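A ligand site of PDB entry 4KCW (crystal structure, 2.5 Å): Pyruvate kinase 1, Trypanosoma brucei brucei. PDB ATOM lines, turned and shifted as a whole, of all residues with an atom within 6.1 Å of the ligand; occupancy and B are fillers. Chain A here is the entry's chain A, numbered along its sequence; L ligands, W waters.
Merely in contact with the ligand: Arg 405, His 481, Val 486, Lys 487, Tyr 489 and Pro 490.
Hydrophobic or aromatic side chains that line the ligand: Leu 400, His 481, Ala 482 and Pro 490.
Of the 25 residues printed, 15 come within 4 Å of the ligand.
Water W3 lies within hydrogen-bond range of O12 of the ligand (2.6 Å), O of Gly 488 (2.8 Å) and NH1 of Arg 405 (3.3 Å).
The side-chain hydroxyl (OG) of Ser 401 lies within hydrogen-bond range of an oxygen (O10) of the ligand (2.5 Å).
The backbone NH of Ser 406 is in hydrogen-bond range of an oxygen (O10) of the ligand, at 2.9 Å.
The side-chain hydroxyl (OG) of Ser 406 is in hydrogen-bond range of an oxygen (O10) of the ligand.
The guanidinium group (NH1) of Arg 457 is in salt-bridge range of an oxygen (O2) of the ligand (2.7 Å).
The backbone NH of Asn 402 sits at hydrogen-bond distance from an oxygen (O11) of the ligand.
The side-chain amide nitrogen (ND2) of Asn 402 is in hydrogen-bond range of an oxygen (O2) of the ligand, at 3.0 Å.
O4 of the ligand sits at hydrogen-bond distance from N of Gly 488, 2.7 Å away.
The backbone carbonyl oxygen of Leu 400 lies within hydrogen-bond range of an oxygen (O7) of the ligand, 2.7 Å away.
The backbone NH (N) of Thr 403 lies within hydrogen-bond range of an oxygen (O11) of the ligand (2.8 Å).
OG1 of Thr 403 is in hydrogen-bond range of O12 of the ligand (3.0 Å).
NZ of Lys 454 is in salt-bridge range of O1 of the ligand (2.8 Å).
N of Ala 482 lies within hydrogen-bond range of O6 of the ligand (3.1 Å).
N of Ser 406 lies within hydrogen-bond range of OG of Ser 401 (3.4 Å).
OG of Ser 401 sits at hydrogen-bond distance from N of Arg 405 (3.3 Å).
The side-chain hydroxyl (OG) of Ser 401 lies within hydrogen-bond range of the backbone NH (N) of Gly 404, at 2.9 Å.
The side-chain amide oxygen (OD1) of Asn 402 sits at hydrogen-bond distance from the side-chain hydroxyl (OG1) of Thr 424 (2.8 Å).
N of Leu 400 is in hydrogen-bond range of O of Val 480 (3.3 Å).
The side-chain amino group of Lys 454 is in hydrogen-bond range of the backbone carbonyl oxygen of Lys 452, 3.0 Å away.
The backbone NH (N) of Asn 491 lies within hydrogen-bond range of the backbone carbonyl oxygen (O) of His 481 (3.3 Å).
N of Val 486 lies within hydrogen-bond range of OD1 of Asp 483.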
ATOM      1  N   VAL A 399     -35.387 -23.221 -23.822  1.00  0.00           N
ATOM      2  CA  VAL A 399     -34.738 -22.181 -23.079  1.00  0.00           C
ATOM      3  C   VAL A 399     -33.218 -22.264 -23.244  1.00  0.00           C
ATOM      4  O   VAL A 399     -32.652 -23.360 -23.253  1.00  0.00           O
ATOM      5  CB  VAL A 399     -35.105 -22.275 -21.608  1.00  0.00           C
ATOM      6  CG1 VAL A 399     -34.720 -23.654 -21.069  1.00  0.00           C
ATOM      7  CG2 VAL A 399     -34.496 -21.123 -20.803  1.00  0.00           C
ATOM      8  N   LEU A 400     -32.581 -21.121 -23.475  1.00  0.00           N
ATOM      9  CA  LEU A 400     -31.140 -21.018 -23.414  1.00  0.00           C
ATOM     10  C   LEU A 400     -30.677 -20.828 -21.985  1.00  0.00           C
ATOM     11  O   LEU A 400     -31.045 -19.842 -21.304  1.00  0.00           O
ATOM     12  CB  LEU A 400     -30.628 -19.865 -24.285  1.00  0.00           C
ATOM     13  CG  LEU A 400     -30.490 -20.154 -25.791  1.00  0.00           C
ATOM     14  CD1 LEU A 400     -31.671 -20.944 -26.281  1.00  0.00           C
ATOM     15  CD2 LEU A 400     -30.314 -18.851 -26.580  1.00  0.00           C
ATOM     16  N   SER A 401     -29.847 -21.742 -21.525  1.00  0.00           N
ATOM     17  CA  SER A 401     -29.297 -21.637 -20.180  1.00  0.00           C
ATOM     18  C   SER A 401     -27.860 -22.092 -20.164  1.00  0.00           C
ATOM     19  O   SER A 401     -27.547 -23.234 -20.549  1.00  0.00           O
ATOM     20  CB  SER A 401     -30.122 -22.467 -19.164  1.00  0.00           C
ATOM     21  OG  SER A 401     -29.799 -22.106 -17.826  1.00  0.00           O
ATOM     22  N   ASN A 402     -26.991 -21.269 -19.626  1.00  0.00           N
ATOM     23  CA  ASN A 402     -25.594 -21.645 -19.516  1.00  0.00           C
ATOM     24  C   ASN A 402     -25.271 -22.281 -18.163  1.00  0.00           C
ATOM     25  O   ASN A 402     -24.555 -23.302 -18.107  1.00  0.00           O
ATOM     26  CB  ASN A 402     -24.714 -20.443 -19.823  1.00  0.00           C
ATOM     27  CG  ASN A 402     -25.032 -19.825 -21.169  1.00  0.00           C
ATOM     28  OD1 ASN A 402     -25.179 -20.564 -22.145  1.00  0.00           O
ATOM     29  ND2 ASN A 402     -25.405 -18.536 -21.169  1.00  0.00           N
ATOM     30  N   THR A 403     -25.865 -21.749 -17.092  1.00  0.00           N
ATOM     31  CA  THR A 403     -25.587 -22.259 -15.752  1.00  0.00           C
ATOM     32  C   THR A 403     -26.613 -23.310 -15.408  1.00  0.00           C
ATOM     33  O   THR A 403     -26.390 -24.150 -14.524  1.00  0.00           O
ATOM     34  CB  THR A 403     -25.654 -21.145 -14.682  1.00  0.00           C
ATOM     35  OG1 THR A 403     -27.008 -20.653 -14.602  1.00  0.00           O
ATOM     36  CG2 THR A 403     -24.702 -19.999 -15.011  1.00  0.00           C
ATOM     37  N   GLY A 404     -27.765 -23.256 -16.106  1.00  0.00           N
ATOM     38  CA  GLY A 404     -28.901 -24.094 -15.763  1.00  0.00           C
ATOM     39  C   GLY A 404     -29.968 -23.357 -14.979  1.00  0.00           C
ATOM     40  O   GLY A 404     -31.087 -23.847 -14.836  1.00  0.00           O
ATOM     41  N   ARG A 405     -29.654 -22.152 -14.523  1.00  0.00           N
ATOM     42  CA  ARG A 405     -30.579 -21.416 -13.666  1.00  0.00           C
ATOM     43  C   ARG A 405     -31.936 -21.232 -14.341  1.00  0.00           C
ATOM     44  O   ARG A 405     -32.990 -21.526 -13.727  1.00  0.00           O
ATOM     45  CB  ARG A 405     -30.007 -20.063 -13.266  1.00  0.00           C
ATOM     46  CG  ARG A 405     -30.696 -19.460 -12.055  1.00  0.00           C
ATOM     47  CD  ARG A 405     -30.612 -17.950 -12.030  1.00  0.00           C
ATOM     48  NE  ARG A 405     -31.666 -17.367 -11.194  1.00  0.00           N
ATOM     49  CZ  ARG A 405     -32.212 -16.173 -11.409  1.00  0.00           C
ATOM     50  NH1 ARG A 405     -31.804 -15.453 -12.448  1.00  0.00           N
ATOM     51  NH2 ARG A 405     -33.141 -15.705 -10.587  1.00  0.00           N
ATOM     52  N   SER A 406     -31.930 -20.779 -15.599  1.00  0.00           N
ATOM     53  CA  SER A 406     -33.188 -20.464 -16.259  1.00  0.00           C
ATOM     54  C   SER A 406     -33.987 -21.714 -16.547  1.00  0.00           C
ATOM     55  O   SER A 406     -35.207 -21.705 -16.412  1.00  0.00           O
ATOM     56  CB  SER A 406     -32.962 -19.659 -17.528  1.00  0.00           C
ATOM     57  OG  SER A 406     -32.120 -18.539 -17.264  1.00  0.00           O
ATOM     58  N   ALA A 407     -33.308 -22.836 -16.790  1.00  0.00           N
ATOM     59  CA  ALA A 407     -34.031 -24.094 -17.008  1.00  0.00           C
ATOM     60  C   ALA A 407     -34.670 -24.626 -15.713  1.00  0.00           C
ATOM     61  O   ALA A 407     -35.810 -25.117 -15.732  1.00  0.00           O
ATOM     62  CB  ALA A 407     -33.135 -25.142 -17.648  1.00  0.00           C
ATOM     63  N   THR A 424     -24.365 -24.026 -23.046  1.00  0.00           N
ATOM     64  CA  THR A 424     -23.019 -23.920 -23.549  1.00  0.00           C
ATOM     65  C   THR A 424     -22.022 -24.712 -22.679  1.00  0.00           C
ATOM     66  O   THR A 424     -20.814 -24.674 -22.915  1.00  0.00           O
ATOM     67  CB  THR A 424     -22.589 -22.434 -23.629  1.00  0.00           C
ATOM     68  OG1 THR A 424     -22.688 -21.843 -22.343  1.00  0.00           O
ATOM     69  CG2 THR A 424     -23.477 -21.675 -24.603  1.00  0.00           C
ATOM     70  N   ARG A 425     -22.546 -25.521 -21.763  1.00  0.00           N
ATOM     71  CA  ARG A 425     -21.693 -26.292 -20.853  1.00  0.00           C
ATOM     72  C   ARG A 425     -22.162 -27.719 -20.708  1.00  0.00           C
ATOM     73  O   ARG A 425     -23.300 -27.995 -20.275  1.00  0.00           O
ATOM     74  CB  ARG A 425     -21.649 -25.638 -19.476  1.00  0.00           C
ATOM     75  CG  ARG A 425     -20.888 -24.333 -19.424  1.00  0.00           C
ATOM     76  CD  ARG A 425     -20.914 -23.745 -18.025  1.00  0.00           C
ATOM     77  NE  ARG A 425     -21.125 -22.302 -18.112  1.00  0.00           N
ATOM     78  CZ  ARG A 425     -21.142 -21.462 -17.072  1.00  0.00           C
ATOM     79  NH1 ARG A 425     -20.929 -21.919 -15.837  1.00  0.00           N
ATOM     80  NH2 ARG A 425     -21.383 -20.172 -17.281  1.00  0.00           N
ATOM     81  N   ASP A 451     -22.753 -16.664 -31.172  1.00  0.00           N
ATOM     82  CA  ASP A 451     -24.234 -16.682 -31.156  1.00  0.00           C
ATOM     83  C   ASP A 451     -24.909 -15.558 -30.353  1.00  0.00           C
ATOM     84  O   ASP A 451     -25.890 -15.802 -29.658  1.00  0.00           O
ATOM     85  CB  ASP A 451     -24.755 -18.038 -30.697  1.00  0.00           C
ATOM     86  CG  ASP A 451     -26.157 -18.352 -31.257  1.00  0.00           C
ATOM     87  OD1 ASP A 451     -26.463 -17.890 -32.382  1.00  0.00           O
ATOM     88  OD2 ASP A 451     -26.920 -19.107 -30.579  1.00  0.00           O
ATOM     89  N   LYS A 452     -24.457 -14.330 -30.549  1.00  0.00           N
ATOM     90  CA  LYS A 452     -24.984 -13.190 -29.783  1.00  0.00           C
ATOM     91  C   LYS A 452     -26.478 -13.052 -29.986  1.00  0.00           C
ATOM     92  O   LYS A 452     -27.194 -12.729 -29.060  1.00  0.00           O
ATOM     93  CB  LYS A 452     -24.286 -11.898 -30.187  1.00  0.00           C
ATOM     94  CG  LYS A 452     -22.769 -11.946 -30.054  1.00  0.00           C
ATOM     95  CD  LYS A 452     -22.194 -10.664 -29.465  1.00  0.00           C
ATOM     96  CE  LYS A 452     -21.125 -10.996 -28.420  1.00  0.00           C
ATOM     97  NZ  LYS A 452     -19.930 -10.123 -28.567  1.00  0.00           N
ATOM     98  N   LYS A 454     -28.532 -15.472 -30.724  1.00  0.00           N
ATOM     99  CA  LYS A 454     -29.215 -16.690 -30.251  1.00  0.00           C
ATOM    100  C   LYS A 454     -29.810 -17.546 -31.361  1.00  0.00           C
ATOM    101  O   LYS A 454     -30.386 -18.579 -31.116  1.00  0.00           O
ATOM    102  CB  LYS A 454     -30.296 -16.415 -29.161  1.00  0.00           C
ATOM    103  CG  LYS A 454     -30.328 -15.011 -28.603  1.00  0.00           C
ATOM    104  CD  LYS A 454     -29.208 -14.787 -27.615  1.00  0.00           C
ATOM    105  CE  LYS A 454     -29.438 -13.512 -26.819  1.00  0.00           C
ATOM    106  NZ  LYS A 454     -28.138 -13.099 -26.213  1.00  0.00           N
ATOM    107  N   ARG A 457     -28.424 -21.250 -31.503  1.00  0.00           N
ATOM    108  CA  ARG A 457     -28.838 -22.092 -30.403  1.00  0.00           C
ATOM    109  C   ARG A 457     -30.310 -22.404 -30.470  1.00  0.00           C
ATOM    110  O   ARG A 457     -30.708 -23.561 -30.301  1.00  0.00           O
ATOM    111  CB  ARG A 457     -28.489 -21.449 -29.068  1.00  0.00           C
ATOM    112  CG  ARG A 457     -27.018 -21.608 -28.727  1.00  0.00           C
ATOM    113  CD  ARG A 457     -26.663 -20.856 -27.487  1.00  0.00           C
ATOM    114  NE  ARG A 457     -26.588 -19.444 -27.742  1.00  0.00           N
ATOM    115  CZ  ARG A 457     -26.549 -18.518 -26.779  1.00  0.00           C
ATOM    116  NH1 ARG A 457     -26.656 -18.892 -25.506  1.00  0.00           N
ATOM    117  NH2 ARG A 457     -26.445 -17.213 -27.077  1.00  0.00           N
ATOM    118  N   VAL A 480     -37.603 -19.150 -24.772  1.00  0.00           N
ATOM    119  CA  VAL A 480     -37.228 -18.217 -23.708  1.00  0.00           C
ATOM    120  C   VAL A 480     -35.727 -17.961 -23.753  1.00  0.00           C
ATOM    121  O   VAL A 480     -34.943 -18.894 -23.688  1.00  0.00           O
ATOM    122  CB  VAL A 480     -37.641 -18.764 -22.325  1.00  0.00           C
ATOM    123  CG1 VAL A 480     -37.020 -17.950 -21.197  1.00  0.00           C
ATOM    124  CG2 VAL A 480     -39.135 -18.753 -22.192  1.00  0.00           C
ATOM    125  N   HIS A 481     -35.341 -16.718 -24.005  1.00  0.00           N
ATOM    126  CA  HIS A 481     -33.948 -16.268 -23.778  1.00  0.00           C
ATOM    127  C   HIS A 481     -33.888 -14.764 -23.635  1.00  0.00           C
ATOM    128  O   HIS A 481     -34.910 -14.117 -23.411  1.00  0.00           O
ATOM    129  CB  HIS A 481     -33.050 -16.730 -24.911  1.00  0.00           C
ATOM    130  CG  HIS A 481     -33.609 -16.454 -26.291  1.00  0.00           C
ATOM    131  ND1 HIS A 481     -33.561 -15.215 -26.866  1.00  0.00           N
ATOM    132  CD2 HIS A 481     -34.165 -17.318 -27.247  1.00  0.00           C
ATOM    133  CE1 HIS A 481     -34.124 -15.268 -28.094  1.00  0.00           C
ATOM    134  NE2 HIS A 481     -34.467 -16.566 -28.338  1.00  0.00           N
ATOM    135  N   ALA A 482     -32.702 -14.173 -23.790  1.00  0.00           N
ATOM    136  CA  ALA A 482     -32.605 -12.696 -23.714  1.00  0.00           C
ATOM    137  C   ALA A 482     -32.884 -12.100 -25.090  1.00  0.00           C
ATOM    138  O   ALA A 482     -32.715 -12.766 -26.096  1.00  0.00           O
ATOM    139  CB  ALA A 482     -31.227 -12.264 -23.205  1.00  0.00           C
ATOM    140  N   ASP A 483     -33.294 -10.841 -25.141  1.00  0.00           N
ATOM    141  CA  ASP A 483     -33.243 -10.099 -26.393  1.00  0.00           C
ATOM    142  C   ASP A 483     -31.794  -9.782 -26.793  1.00  0.00           C
ATOM    143  O   ASP A 483     -30.854 -10.339 -26.223  1.00  0.00           O
ATOM    144  CB  ASP A 483     -34.100  -8.809 -26.308  1.00  0.00           C
ATOM    145  CG  ASP A 483     -33.561  -7.762 -25.294  1.00  0.00           C
ATOM    146  OD1 ASP A 483     -32.330  -7.667 -25.045  1.00  0.00           O
ATOM    147  OD2 ASP A 483     -34.374  -6.945 -24.857  1.00  0.00           O
ATOM    148  N   VAL A 486     -29.677  -7.714 -23.531  1.00  0.00           N
ATOM    149  CA  VAL A 486     -29.627  -8.037 -22.115  1.00  0.00           C
ATOM    150  C   VAL A 486     -28.713  -9.213 -21.855  1.00  0.00           C
ATOM    151  O   VAL A 486     -28.689 -10.162 -22.632  1.00  0.00           O
ATOM    152  CB  VAL A 486     -31.033  -8.281 -21.556  1.00  0.00           C
ATOM    153  CG1 VAL A 486     -30.971  -8.881 -20.154  1.00  0.00           C
ATOM    154  CG2 VAL A 486     -31.841  -6.990 -21.590  1.00  0.00           C
ATOM    155  N   LYS A 487     -27.841  -9.083 -20.849  1.00  0.00           N
ATOM    156  CA  LYS A 487     -26.911 -10.145 -20.502  1.00  0.00           C
ATOM    157  C   LYS A 487     -27.180 -10.612 -19.094  1.00  0.00           C
ATOM    158  O   LYS A 487     -27.419  -9.799 -18.203  1.00  0.00           O
ATOM    159  CB  LYS A 487     -25.460  -9.650 -20.634  1.00  0.00           C
ATOM    160  CG  LYS A 487     -25.123  -9.145 -22.018  1.00  0.00           C
ATOM    161  CD  LYS A 487     -24.862 -10.293 -22.993  1.00  0.00           C
ATOM    162  CE  LYS A 487     -24.368  -9.779 -24.348  1.00  0.00           C
ATOM    163  NZ  LYS A 487     -25.395  -9.908 -25.446  1.00  0.00           N
ATOM    164  N   GLY A 488     -27.212 -11.925 -18.901  1.00  0.00           N
ATOM    165  CA  GLY A 488     -27.165 -12.479 -17.569  1.00  0.00           C
ATOM    166  C   GLY A 488     -28.427 -13.221 -17.146  1.00  0.00           C
ATOM    167  O   GLY A 488     -28.439 -13.919 -16.127  1.00  0.00           O
ATOM    168  N   TYR A 489     -29.514 -13.047 -17.893  1.00  0.00           N
ATOM    169  CA  TYR A 489     -30.764 -13.712 -17.537  1.00  0.00           C
ATOM    170  C   TYR A 489     -31.686 -13.596 -18.732  1.00  0.00           C
ATOM    171  O   TYR A 489     -31.390 -12.844 -19.637  1.00  0.00           O
ATOM    172  CB  TYR A 489     -31.387 -13.044 -16.288  1.00  0.00           C
ATOM    173  CG  TYR A 489     -31.747 -11.586 -16.493  1.00  0.00           C
ATOM    174  CD1 TYR A 489     -30.806 -10.557 -16.278  1.00  0.00           C
ATOM    175  CD2 TYR A 489     -33.009 -11.224 -17.025  1.00  0.00           C
ATOM    176  CE1 TYR A 489     -31.114  -9.216 -16.564  1.00  0.00           C
ATOM    177  CE2 TYR A 489     -33.340  -9.896 -17.273  1.00  0.00           C
ATOM    178  CZ  TYR A 489     -32.391  -8.899 -17.032  1.00  0.00           C
ATOM    179  OH  TYR A 489     -32.755  -7.593 -17.255  1.00  0.00           O
ATOM    180  N   PRO A 490     -32.766 -14.392 -18.785  1.00  0.00           N
ATOM    181  CA  PRO A 490     -33.622 -14.207 -19.959  1.00  0.00           C
ATOM    182  C   PRO A 490     -34.647 -13.127 -19.695  1.00  0.00           C
ATOM    183  O   PRO A 490     -35.256 -13.082 -18.619  1.00  0.00           O
ATOM    184  CB  PRO A 490     -34.320 -15.553 -20.075  1.00  0.00           C
ATOM    185  CG  PRO A 490     -34.347 -16.074 -18.693  1.00  0.00           C
ATOM    186  CD  PRO A 490     -33.045 -15.647 -18.084  1.00  0.00           C
ATOM    187  N   ASN A 491     -34.845 -12.227 -20.646  1.00  0.00           N
ATOM    188  CA  ASN A 491     -35.860 -11.187 -20.436  1.00  0.00           C
ATOM    189  C   ASN A 491     -36.984 -11.257 -21.482  1.00  0.00           C
ATOM    190  O   ASN A 491     -37.799 -10.363 -21.570  1.00  0.00           O
ATOM    191  CB  ASN A 491     -35.206  -9.789 -20.413  1.00  0.00           C
ATOM    192  CG  ASN A 491     -34.774  -9.332 -21.785  1.00  0.00           C
ATOM    193  OD1 ASN A 491     -34.219 -10.118 -22.570  1.00  0.00           O
ATOM    194  ND2 ASN A 491     -35.204  -8.146 -22.164  1.00  0.00           N
HETATM  195  P1  LIG L   1     -26.683 -15.736 -23.640  1.00  0.00           P
HETATM  196  O1  LIG L   1     -27.459 -15.462 -24.842  1.00  0.00           O
HETATM  197  O2  LIG L   1     -25.834 -17.038 -23.753  1.00  0.00           O
HETATM  198  O3  LIG L   1     -25.688 -14.577 -23.238  1.00  0.00           O
HETATM  199  O4  LIG L   1     -26.997 -13.352 -21.194  1.00  0.00           O
HETATM  200  C1  LIG L   1     -28.059 -13.667 -22.117  1.00  0.00           C
HETATM  201  C2  LIG L   1     -28.522 -15.106 -21.832  1.00  0.00           C
HETATM  202  O5  LIG L   1     -27.575 -16.006 -22.321  1.00  0.00           O
HETATM  203  C3  LIG L   1     -29.927 -15.425 -22.345  1.00  0.00           C
HETATM  204  O6  LIG L   1     -29.959 -15.596 -23.764  1.00  0.00           O
HETATM  205  C4  LIG L   1     -30.102 -16.745 -21.656  1.00  0.00           C
HETATM  206  O7  LIG L   1     -31.486 -17.158 -21.703  1.00  0.00           O
HETATM  207  C5  LIG L   1     -29.649 -16.401 -20.226  1.00  0.00           C
HETATM  208  O8  LIG L   1     -28.655 -15.349 -20.395  1.00  0.00           O
HETATM  209  C6  LIG L   1     -29.015 -17.637 -19.571  1.00  0.00           C
HETATM  210  O9  LIG L   1     -28.851 -17.456 -18.160  1.00  0.00           O
HETATM  211  P2  LIG L   1     -28.608 -18.701 -17.193  1.00  0.00           P
HETATM  212  O10 LIG L   1     -29.782 -19.667 -17.133  1.00  0.00           O
HETATM  213  O11 LIG L   1     -27.260 -19.395 -17.716  1.00  0.00           O
HETATM  214  O12 LIG L   1     -28.253 -18.124 -15.715  1.00  0.00           O
HETATM  215  O   HOH W   1     -24.121 -13.605 -19.509  1.00  0.00           O
HETATM  216  O   HOH W   2     -23.411 -14.376 -22.083  1.00  0.00           O
HETATM  217  O   HOH W   3     -29.838 -16.142 -15.060  1.00  0.00           O
